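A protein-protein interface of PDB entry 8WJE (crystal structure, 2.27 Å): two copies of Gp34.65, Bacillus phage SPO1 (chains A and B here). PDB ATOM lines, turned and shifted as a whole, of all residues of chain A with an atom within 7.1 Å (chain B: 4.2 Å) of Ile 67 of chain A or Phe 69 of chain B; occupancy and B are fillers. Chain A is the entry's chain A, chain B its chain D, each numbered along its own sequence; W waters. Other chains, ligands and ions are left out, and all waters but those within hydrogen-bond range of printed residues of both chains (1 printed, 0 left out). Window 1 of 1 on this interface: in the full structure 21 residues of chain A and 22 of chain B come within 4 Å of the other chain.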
ATOM      1  N   PHE A  40     -17.797  13.922  -8.155  1.00  0.00           N
ATOM      2  CA  PHE A  40     -17.732  13.162  -6.918  1.00  0.00           C
ATOM      3  C   PHE A  40     -16.272  12.891  -6.634  1.00  0.00           C
ATOM      4  O   PHE A  40     -15.421  12.978  -7.527  1.00  0.00           O
ATOM      5  CB  PHE A  40     -18.577  11.863  -6.974  1.00  0.00           C
ATOM      6  CG  PHE A  40     -18.101  10.817  -7.997  1.00  0.00           C
ATOM      7  CD1 PHE A  40     -18.531  10.863  -9.314  1.00  0.00           C
ATOM      8  CD2 PHE A  40     -17.246   9.781  -7.625  1.00  0.00           C
ATOM      9  CE1 PHE A  40     -18.117   9.911 -10.235  1.00  0.00           C
ATOM     10  CE2 PHE A  40     -16.807   8.797  -8.585  1.00  0.00           C
ATOM     11  CZ  PHE A  40     -17.246   8.884  -9.861  1.00  0.00           C
ATOM     12  N   LEU A  41     -15.982  12.594  -5.383  1.00  0.00           N
ATOM     13  CA  LEU A  41     -14.626  12.400  -4.885  1.00  0.00           C
ATOM     14  C   LEU A  41     -14.437  10.925  -4.567  1.00  0.00           C
ATOM     15  O   LEU A  41     -15.097  10.395  -3.676  1.00  0.00           O
ATOM     16  CB  LEU A  41     -14.386  13.236  -3.630  1.00  0.00           C
ATOM     17  CG  LEU A  41     -13.020  12.979  -2.998  1.00  0.00           C
ATOM     18  CD1 LEU A  41     -11.915  13.603  -3.842  1.00  0.00           C
ATOM     19  CD2 LEU A  41     -13.009  13.578  -1.620  1.00  0.00           C
ATOM     20  N   LYS A  42     -13.539  10.261  -5.276  1.00  0.00           N
ATOM     21  CA  LYS A  42     -13.098   8.930  -4.914  1.00  0.00           C
ATOM     22  C   LYS A  42     -11.904   9.068  -3.985  1.00  0.00           C
ATOM     23  O   LYS A  42     -10.881   9.645  -4.365  1.00  0.00           O
ATOM     24  CB  LYS A  42     -12.706   8.128  -6.143  1.00  0.00           C
ATOM     25  CG  LYS A  42     -12.464   6.705  -5.695  1.00  0.00           C
ATOM     26  CD  LYS A  42     -12.720   5.690  -6.769  1.00  0.00           C
ATOM     27  CE  LYS A  42     -11.437   5.216  -7.415  1.00  0.00           C
ATOM     28  NZ  LYS A  42     -11.499   3.715  -7.521  1.00  0.00           N
ATOM     29  N   SER A  43     -12.045   8.607  -2.757  1.00  0.00           N
ATOM     30  CA  SER A  43     -10.929   8.714  -1.836  1.00  0.00           C
ATOM     31  C   SER A  43      -9.878   7.651  -2.202  1.00  0.00           C
ATOM     32  O   SER A  43     -10.132   6.735  -2.987  1.00  0.00           O
ATOM     33  CB  SER A  43     -11.413   8.560  -0.392  1.00  0.00           C
ATOM     34  OG  SER A  43     -10.339   8.705   0.512  1.00  0.00           O
ATOM     35  N   SER A  44      -8.675   7.811  -1.670  1.00  0.00           N
ATOM     36  CA  SER A  44      -7.562   6.937  -2.007  1.00  0.00           C
ATOM     37  C   SER A  44      -7.896   5.468  -1.799  1.00  0.00           C
ATOM     38  O   SER A  44      -8.223   5.066  -0.688  1.00  0.00           O
ATOM     39  CB  SER A  44      -6.385   7.344  -1.140  1.00  0.00           C
ATOM     40  OG  SER A  44      -5.345   6.390  -1.225  1.00  0.00           O
ATOM     41  N   PHE A  64      -3.093   5.024  -5.656  1.00  0.00           N
ATOM     42  CA  PHE A  64      -4.008   6.072  -6.104  1.00  0.00           C
ATOM     43  C   PHE A  64      -4.441   6.928  -4.933  1.00  0.00           C
ATOM     44  O   PHE A  64      -4.981   6.405  -3.967  1.00  0.00           O
ATOM     45  CB  PHE A  64      -5.219   5.452  -6.768  1.00  0.00           C
ATOM     46  CG  PHE A  64      -4.895   4.875  -8.085  1.00  0.00           C
ATOM     47  CD1 PHE A  64      -4.846   5.672  -9.193  1.00  0.00           C
ATOM     48  CD2 PHE A  64      -4.562   3.551  -8.197  1.00  0.00           C
ATOM     49  CE1 PHE A  64      -4.496   5.167 -10.432  1.00  0.00           C
ATOM     50  CE2 PHE A  64      -4.206   3.011  -9.414  1.00  0.00           C
ATOM     51  CZ  PHE A  64      -4.172   3.819 -10.556  1.00  0.00           C
ATOM     52  N   GLY A  65      -4.181   8.234  -5.004  1.00  0.00           N
ATOM     53  CA  GLY A  65      -4.681   9.168  -4.013  1.00  0.00           C
ATOM     54  C   GLY A  65      -6.116   9.542  -4.340  1.00  0.00           C
ATOM     55  O   GLY A  65      -6.765   8.940  -5.197  1.00  0.00           O
ATOM     56  N   ASN A  66      -6.609  10.581  -3.667  1.00  0.00           N
ATOM     57  CA  ASN A  66      -7.946  11.093  -3.958  1.00  0.00           C
ATOM     58  C   ASN A  66      -8.074  11.539  -5.386  1.00  0.00           C
ATOM     59  O   ASN A  66      -7.196  12.205  -5.931  1.00  0.00           O
ATOM     60  CB  ASN A  66      -8.274  12.330  -3.137  1.00  0.00           C
ATOM     61  CG  ASN A  66      -8.173  12.091  -1.720  1.00  0.00           C
ATOM     62  OD1 ASN A  66      -8.781  11.125  -1.168  1.00  0.00           O
ATOM     63  ND2 ASN A  66      -7.387  12.963  -1.064  1.00  0.00           N
ATOM     64  N   ILE A  67      -9.221  11.296  -5.956  1.00  0.00           N
ATOM     65  CA  ILE A  67      -9.436  11.756  -7.303  1.00  0.00           C
ATOM     66  C   ILE A  67     -10.826  12.334  -7.390  1.00  0.00           C
ATOM     67  O   ILE A  67     -11.797  11.693  -6.977  1.00  0.00           O
ATOM     68  CB  ILE A  67      -9.292  10.600  -8.308  1.00  0.00           C
ATOM     69  CG1 ILE A  67      -7.878  10.010  -8.257  1.00  0.00           C
ATOM     70  CG2 ILE A  67      -9.720  11.086  -9.673  1.00  0.00           C
ATOM     71  CD1 ILE A  67      -7.818   8.614  -9.002  1.00  0.00           C
ATOM     72  N   ILE A  68     -10.943  13.484  -7.975  1.00  0.00           N
ATOM     73  CA  ILE A  68     -12.254  14.041  -8.250  1.00  0.00           C
ATOM     74  C   ILE A  68     -12.614  13.652  -9.653  1.00  0.00           C
ATOM     75  O   ILE A  68     -11.860  13.915 -10.589  1.00  0.00           O
ATOM     76  CB  ILE A  68     -12.258  15.571  -8.110  1.00  0.00           C
ATOM     77  CG1 ILE A  68     -11.555  15.971  -6.859  1.00  0.00           C
ATOM     78  CG2 ILE A  68     -13.656  16.123  -8.169  1.00  0.00           C
ATOM     79  CD1 ILE A  68     -11.257  17.462  -6.849  1.00  0.00           C
ATOM     80  N   PHE A  69     -13.782  13.071  -9.799  1.00  0.00           N
ATOM     81  CA  PHE A  69     -14.332  12.659 -11.064  1.00  0.00           C
ATOM     82  C   PHE A  69     -15.492  13.557 -11.427  1.00  0.00           C
ATOM     83  O   PHE A  69     -16.189  14.104 -10.563  1.00  0.00           O
ATOM     84  CB  PHE A  69     -14.811  11.205 -10.998  1.00  0.00           C
ATOM     85  CG  PHE A  69     -13.716  10.240 -10.894  1.00  0.00           C
ATOM     86  CD1 PHE A  69     -12.889  10.010 -11.988  1.00  0.00           C
ATOM     87  CD2 PHE A  69     -13.486   9.544  -9.721  1.00  0.00           C
ATOM     88  CE1 PHE A  69     -11.840   9.107 -11.911  1.00  0.00           C
ATOM     89  CE2 PHE A  69     -12.423   8.618  -9.649  1.00  0.00           C
ATOM     90  CZ  PHE A  69     -11.604   8.422 -10.738  1.00  0.00           C
ATOM     91  N   HIS A  78     -14.805  10.869 -16.032  1.00  0.00           N
ATOM     92  CA  HIS A  78     -13.483  11.406 -16.318  1.00  0.00           C
ATOM     93  C   HIS A  78     -12.904  12.079 -15.082  1.00  0.00           C
ATOM     94  O   HIS A  78     -13.633  12.504 -14.187  1.00  0.00           O
ATOM     95  CB  HIS A  78     -13.534  12.408 -17.431  1.00  0.00           C
ATOM     96  CG  HIS A  78     -14.010  11.830 -18.713  1.00  0.00           C
ATOM     97  ND1 HIS A  78     -15.242  12.131 -19.251  1.00  0.00           N
ATOM     98  CD2 HIS A  78     -13.439  10.930 -19.545  1.00  0.00           C
ATOM     99  CE1 HIS A  78     -15.410  11.447 -20.363  1.00  0.00           C
ATOM    100  NE2 HIS A  78     -14.334  10.708 -20.561  1.00  0.00           N
ATOM    101  N   ALA A  79     -11.584  12.154 -15.021  1.00  0.00           N
ATOM    102  CA  ALA A  79     -10.941  12.977 -14.015  1.00  0.00           C
ATOM    103  C   ALA A  79     -11.299  14.435 -14.250  1.00  0.00           C
ATOM    104  O   ALA A  79     -11.244  14.911 -15.380  1.00  0.00           O
ATOM    105  CB  ALA A  79      -9.446  12.812 -14.085  1.00  0.00           C
ATOM    106  N   TRP A  80     -11.639  15.161 -13.176  1.00  0.00           N
ATOM    107  CA  TRP A  80     -12.096  16.533 -13.308  1.00  0.00           C
ATOM    108  C   TRP A  80     -10.937  17.512 -13.353  1.00  0.00           C
ATOM    109  O   TRP A  80     -10.025  17.471 -12.518  1.00  0.00           O
ATOM    110  CB  TRP A  80     -12.985  16.913 -12.155  1.00  0.00           C
ATOM    111  CG  TRP A  80     -13.563  18.221 -12.297  1.00  0.00           C
ATOM    112  CD1 TRP A  80     -14.262  18.669 -13.350  1.00  0.00           C
ATOM    113  CD2 TRP A  80     -13.531  19.279 -11.333  1.00  0.00           C
ATOM    114  NE1 TRP A  80     -14.661  19.951 -13.128  1.00  0.00           N
ATOM    115  CE2 TRP A  80     -14.257  20.337 -11.874  1.00  0.00           C
ATOM    116  CE3 TRP A  80     -12.989  19.407 -10.057  1.00  0.00           C
ATOM    117  CZ2 TRP A  80     -14.440  21.525 -11.211  1.00  0.00           C
ATOM    118  CZ3 TRP A  80     -13.151  20.585  -9.394  1.00  0.00           C
ATOM    119  CH2 TRP A  80     -13.889  21.631  -9.961  1.00  0.00           C
ATOM    120  N   PHE B  38       5.912  10.940 -13.653  1.00  0.00           N
ATOM    121  CA  PHE B  38       5.546  10.732 -14.990  1.00  0.00           C
ATOM    122  C   PHE B  38       4.107  10.626 -15.228  1.00  0.00           C
ATOM    123  O   PHE B  38       3.361  10.344 -14.350  1.00  0.00           O
ATOM    124  CB  PHE B  38       6.186   9.463 -15.550  1.00  0.00           C
ATOM    125  CG  PHE B  38       5.858   8.224 -14.806  1.00  0.00           C
ATOM    126  CD1 PHE B  38       6.646   7.820 -13.759  1.00  0.00           C
ATOM    127  CD2 PHE B  38       4.787   7.447 -15.180  1.00  0.00           C
ATOM    128  CE1 PHE B  38       6.359   6.680 -13.073  1.00  0.00           C
ATOM    129  CE2 PHE B  38       4.491   6.302 -14.497  1.00  0.00           C
ATOM    130  CZ  PHE B  38       5.286   5.923 -13.447  1.00  0.00           C
ATOM    131  N   LEU B  39       3.725  10.874 -16.443  1.00  0.00           N
ATOM    132  CA  LEU B  39       2.340  10.662 -16.824  1.00  0.00           C
ATOM    133  C   LEU B  39       2.148   9.259 -17.391  1.00  0.00           C
ATOM    134  O   LEU B  39       3.067   8.687 -17.981  1.00  0.00           O
ATOM    135  CB  LEU B  39       1.911  11.652 -17.896  1.00  0.00           C
ATOM    136  CG  LEU B  39       2.258  13.113 -17.639  1.00  0.00           C
ATOM    137  CD1 LEU B  39       1.518  13.843 -18.720  1.00  0.00           C
ATOM    138  CD2 LEU B  39       1.812  13.554 -16.246  1.00  0.00           C
ATOM    139  N   PHE B  40       0.937   8.725 -17.218  1.00  0.00           N
ATOM    140  CA  PHE B  40       0.493   7.558 -17.952  1.00  0.00           C
ATOM    141  C   PHE B  40      -0.969   7.705 -18.284  1.00  0.00           C
ATOM    142  O   PHE B  40      -1.672   8.547 -17.725  1.00  0.00           O
ATOM    143  CB  PHE B  40       0.747   6.252 -17.212  1.00  0.00           C
ATOM    144  CG  PHE B  40       0.149   6.172 -15.846  1.00  0.00           C
ATOM    145  CD1 PHE B  40       0.789   6.746 -14.757  1.00  0.00           C
ATOM    146  CD2 PHE B  40      -0.997   5.434 -15.631  1.00  0.00           C
ATOM    147  CE1 PHE B  40       0.277   6.641 -13.480  1.00  0.00           C
ATOM    148  CE2 PHE B  40      -1.539   5.319 -14.351  1.00  0.00           C
ATOM    149  CZ  PHE B  40      -0.894   5.925 -13.269  1.00  0.00           C
ATOM    150  N   LYS B  42      -4.636   5.570 -18.744  1.00  0.00           N
ATOM    151  CA  LYS B  42      -5.428   4.353 -18.571  1.00  0.00           C
ATOM    152  C   LYS B  42      -6.722   4.457 -19.350  1.00  0.00           C
ATOM    153  O   LYS B  42      -7.490   5.421 -19.167  1.00  0.00           O
ATOM    154  CB  LYS B  42      -5.799   4.089 -17.119  1.00  0.00           C
ATOM    155  CG  LYS B  42      -4.653   4.138 -16.219  1.00  0.00           C
ATOM    156  CD  LYS B  42      -3.694   3.084 -16.590  1.00  0.00           C
ATOM    157  CE  LYS B  42      -3.967   1.854 -15.828  1.00  0.00           C
ATOM    158  NZ  LYS B  42      -2.667   1.217 -15.546  1.00  0.00           N
ATOM    159  N   LEU B  47      -9.190   0.760 -16.632  1.00  0.00           N
ATOM    160  CA  LEU B  47      -9.590   1.345 -15.346  1.00  0.00           C
ATOM    161  C   LEU B  47     -10.656   0.489 -14.649  1.00  0.00           C
ATOM    162  O   LEU B  47     -10.605   0.298 -13.426  1.00  0.00           O
ATOM    163  CB  LEU B  47     -10.085   2.770 -15.536  1.00  0.00           C
ATOM    164  CG  LEU B  47      -9.055   3.906 -15.706  1.00  0.00           C
ATOM    165  CD1 LEU B  47      -9.740   5.227 -16.146  1.00  0.00           C
ATOM    166  CD2 LEU B  47      -8.250   4.151 -14.444  1.00  0.00           C
ATOM    167  N   PHE B  51      -9.643  -0.328 -10.839  1.00  0.00           N
ATOM    168  CA  PHE B  51     -10.472   0.213  -9.769  1.00  0.00           C
ATOM    169  C   PHE B  51     -11.576  -0.736  -9.340  1.00  0.00           C
ATOM    170  O   PHE B  51     -12.230  -0.472  -8.323  1.00  0.00           O
ATOM    171  CB  PHE B  51     -11.096   1.556 -10.187  1.00  0.00           C
ATOM    172  CG  PHE B  51     -10.084   2.650 -10.404  1.00  0.00           C
ATOM    173  CD1 PHE B  51      -8.742   2.449 -10.092  1.00  0.00           C
ATOM    174  CD2 PHE B  51     -10.470   3.886 -10.909  1.00  0.00           C
ATOM    175  CE1 PHE B  51      -7.794   3.460 -10.304  1.00  0.00           C
ATOM    176  CE2 PHE B  51      -9.523   4.909 -11.114  1.00  0.00           C
ATOM    177  CZ  PHE B  51      -8.186   4.689 -10.800  1.00  0.00           C
ATOM    178  N   ILE B  67      -8.241   8.231 -18.914  1.00  0.00           N
ATOM    179  CA  ILE B  67      -7.805   9.116 -17.864  1.00  0.00           C
ATOM    180  C   ILE B  67      -6.295   9.179 -17.863  1.00  0.00           C
ATOM    181  O   ILE B  67      -5.622   8.144 -17.833  1.00  0.00           O
ATOM    182  CB  ILE B  67      -8.321   8.694 -16.481  1.00  0.00           C
ATOM    183  CG1 ILE B  67      -9.864   8.709 -16.489  1.00  0.00           C
ATOM    184  CG2 ILE B  67      -7.803   9.724 -15.426  1.00  0.00           C
ATOM    185  CD1 ILE B  67     -10.489   8.662 -15.097  1.00  0.00           C
ATOM    186  N   ILE B  68      -5.765  10.397 -17.856  1.00  0.00           N
ATOM    187  CA  ILE B  68      -4.342  10.612 -17.733  1.00  0.00           C
ATOM    188  C   ILE B  68      -4.048  10.826 -16.280  1.00  0.00           C
ATOM    189  O   ILE B  68      -4.657  11.695 -15.641  1.00  0.00           O
ATOM    190  CB  ILE B  68      -3.870  11.830 -18.551  1.00  0.00           C
ATOM    191  CG1 ILE B  68      -4.303  11.700 -20.001  1.00  0.00           C
ATOM    192  CG2 ILE B  68      -2.378  11.984 -18.391  1.00  0.00           C
ATOM    193  CD1 ILE B  68      -4.317  13.007 -20.719  1.00  0.00           C
ATOM    194  N   PHE B  69      -3.061  10.107 -15.782  1.00  0.00           N
ATOM    195  CA  PHE B  69      -2.615  10.198 -14.417  1.00  0.00           C
ATOM    196  C   PHE B  69      -1.185  10.662 -14.389  1.00  0.00           C
ATOM    197  O   PHE B  69      -0.437  10.546 -15.381  1.00  0.00           O
ATOM    198  CB  PHE B  69      -2.676   8.841 -13.732  1.00  0.00           C
ATOM    199  CG  PHE B  69      -4.068   8.290 -13.617  1.00  0.00           C
ATOM    200  CD1 PHE B  69      -4.885   8.661 -12.525  1.00  0.00           C
ATOM    201  CD2 PHE B  69      -4.580   7.432 -14.593  1.00  0.00           C
ATOM    202  CE1 PHE B  69      -6.190   8.166 -12.398  1.00  0.00           C
ATOM    203  CE2 PHE B  69      -5.904   6.899 -14.454  1.00  0.00           C
ATOM    204  CZ  PHE B  69      -6.704   7.281 -13.338  1.00  0.00           C
ATOM    205  N   ILE B  70      -0.804  11.089 -13.210  1.00  0.00           N
ATOM    206  CA  ILE B  70       0.527  11.472 -12.943  1.00  0.00           C
ATOM    207  C   ILE B  70       0.989  10.743 -11.720  1.00  0.00           C
ATOM    208  O   ILE B  70       0.309  10.693 -10.722  1.00  0.00           O
ATOM    209  CB  ILE B  70       0.693  12.998 -12.701  1.00  0.00           C
ATOM    210  CG1 ILE B  70       2.121  13.356 -12.318  1.00  0.00           C
ATOM    211  CG2 ILE B  70      -0.298  13.537 -11.680  1.00  0.00           C
ATOM    212  CD1 ILE B  70       2.450  14.807 -12.559  1.00  0.00           C
ATOM    213  N   ILE B  77      -0.535   8.442  -7.000  1.00  0.00           N
ATOM    214  CA  ILE B  77      -1.108   8.683  -8.277  1.00  0.00           C
ATOM    215  C   ILE B  77      -2.269   9.621  -8.179  1.00  0.00           C
ATOM    216  O   ILE B  77      -3.117   9.456  -7.327  1.00  0.00           O
ATOM    217  CB  ILE B  77      -1.569   7.395  -8.948  1.00  0.00           C
ATOM    218  CG1 ILE B  77      -0.435   6.382  -8.952  1.00  0.00           C
ATOM    219  CG2 ILE B  77      -1.982   7.663 -10.364  1.00  0.00           C
ATOM    220  CD1 ILE B  77      -0.861   4.991  -9.320  1.00  0.00           C
ATOM    221  N   HIS B  78      -2.301  10.617  -9.037  1.00  0.00           N
ATOM    222  CA  HIS B  78      -3.383  11.520  -9.074  1.00  0.00           C
ATOM    223  C   HIS B  78      -3.747  11.721 -10.477  1.00  0.00           C
ATOM    224  O   HIS B  78      -2.948  11.465 -11.346  1.00  0.00           O
ATOM    225  CB  HIS B  78      -3.024  12.831  -8.411  1.00  0.00           C
ATOM    226  CG  HIS B  78      -2.841  12.745  -6.927  1.00  0.00           C
ATOM    227  ND1 HIS B  78      -1.639  12.774  -6.351  1.00  0.00           N
ATOM    228  CD2 HIS B  78      -3.762  12.635  -5.903  1.00  0.00           C
ATOM    229  CE1 HIS B  78      -1.778  12.682  -5.028  1.00  0.00           C
ATOM    230  NE2 HIS B  78      -3.078  12.597  -4.753  1.00  0.00           N
ATOM    231  N   ALA B  79      -4.964  12.150 -10.724  1.00  0.00           N
ATOM    232  CA  ALA B  79      -5.383  12.497 -12.055  1.00  0.00           C
ATOM    233  C   ALA B  79      -4.598  13.723 -12.491  1.00  0.00           C
ATOM    234  O   ALA B  79      -4.326  14.629 -11.701  1.00  0.00           O
ATOM    235  CB  ALA B  79      -6.877  12.773 -12.090  1.00  0.00           C
ATOM    236  N   TRP B  80      -4.195  13.735 -13.746  1.00  0.00           N
ATOM    237  CA  TRP B  80      -3.313  14.779 -14.212  1.00  0.00           C
ATOM    238  C   TRP B  80      -4.101  15.952 -14.746  1.00  0.00           C
ATOM    239  O   TRP B  80      -4.970  15.811 -15.612  1.00  0.00           O
ATOM    240  CB  TRP B  80      -2.390  14.288 -15.299  1.00  0.00           C
ATOM    241  CG  TRP B  80      -1.459  15.360 -15.776  1.00  0.00           C
ATOM    242  CD1 TRP B  80      -0.478  15.987 -15.048  1.00  0.00           C
ATOM    243  CD2 TRP B  80      -1.405  15.903 -17.078  1.00  0.00           C
ATOM    244  NE1 TRP B  80       0.218  16.853 -15.856  1.00  0.00           N
ATOM    245  CE2 TRP B  80      -0.328  16.815 -17.110  1.00  0.00           C
ATOM    246  CE3 TRP B  80      -2.127  15.670 -18.251  1.00  0.00           C
ATOM    247  CZ2 TRP B  80       0.016  17.520 -18.253  1.00  0.00           C
ATOM    248  CZ3 TRP B  80      -1.783  16.375 -19.402  1.00  0.00           C
ATOM    249  CH2 TRP B  80      -0.717  17.297 -19.385  1.00  0.00           C
HETATM  250  O   HOH W   1      -6.231  13.146  -8.366  1.00  0.00           O
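N of Gly 65 of chain A sits at hydrogen-bond distance from O of Ile 77 of chain B.
The backbone carbonyl oxygen of Ile 67 of chain A sits at hydrogen-bond distance from the backbone NH of Lys 42 of chain A (2.8 Å).
The backbone carbonyl oxygen (O) of Phe 40 of chain A sits at hydrogen-bond distance from the backbone NH (N) of Phe 69 of chain A (2.8 Å).
The side-chain hydroxyl (OG) of Ser 44 of chain A lies within hydrogen-bond range of the backbone carbonyl oxygen (O) of Phe 64 of chain A (2.8 Å).
The backbone NH (N) of Ser 44 of chain A sits at hydrogen-bond distance from the side-chain amide oxygen (OD1) of Asn 66 of chain A.
OG of Ser 43 of chain A lies close to OD1 of Asn 66 of chain A, at 3.3 Å.
The backbone NH of Phe 69 of chain B sits at hydrogen-bond distance from the backbone carbonyl oxygen of Phe 40 of chain B (2.9 Å).
Among the printed residues, merely in contact across the chains: Lys 42 of chain A with Phe 51 of chain B (3.4 Å), Phe 64 of chain A with Phe 51 of chain B (3.6 Å), Phe 64 of chain A with Phe 69 of chain B (3.97 Å), Phe 64 of chain A with Ile 77 of chain B (3.5 Å), Gly 65 of chain A with His 78 of chain B (3.9 Å), Asn 66 of chain A with His 78 of chain B (3.5 Å), Ile 67 of chain A with Phe 69 of chain B (3.8 Å), Phe 69 of chain A with Ile 67 of chain B (3.5 Å), Ala 79 of chain A with Ile 67 of chain B (3.7 Å) and Ala 79 of chain A with Ala 79 of chain B (3.3 Å).
Of the printed residues of chain B, Asn 66 of chain A touches His 78 (3.5 Å).
Of chain B, only Phe 69 comes within 4 Å of Ile 67 of chain A.
Printed residues of chain B within 4 Å of Phe 69 of chain A: Ile 67.
Of the printed residues of chain B, Ala 79 of chain A touches Ile 67 and Ala 79.
Leu 39 of chain B touches none of the printed residues of chain A.
Leu 47 of chain B touches none of the printed residues of chain A.
Phe 69 of chain B touches just these residues of chain A: Phe 64 and Ile 67.
Printed residues of chain A within 4 Å of Ile 77 of chain B: Phe 64 and Gly 65.
The nearest residue of chain B that does not touch Ile 67 of chain A is Ala 79 of chain B (4.1 Å).
Of the 14 printed residues of chain A, 7 touch a printed residue of chain B.
Of the 14 printed residues of chain B, 6 touch a printed residue of chain A.
Hydrophobic or aromatic side chains of chain B that line the printed part of chain A: Phe 51, Ile 67, Phe 69, Ile 77, His 78 and Ala 79.
Among the printed residues, 11 pairs touch across the chains.
Among the printed residues, no Asp or Glu carboxylate lies within 4 Å of a Lys or Arg side-chain nitrogen of the other chain.
Ile 67 of chain A touches Phe 69 of chain B, and with the chains exchanged Phe 69 of chain A touches Ile 67 of chain B.
Ala 79 of chain A touches Ile 67 of chain B, but with the chains exchanged Ile 67 of chain A does not touch Ala 79 of chain B (4.1 Å).
Ala 79 of chain B touches its own counterpart, Ala 79 of chain A.
Of the 11 pairs that touch across the chains among the printed residues, 3 have their exchanged pair printed and touching as well.
Water W1 bridges O of Asn 66 of chain A (2.8 Å) and N of Ala 79 of chain B (2.9 Å).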
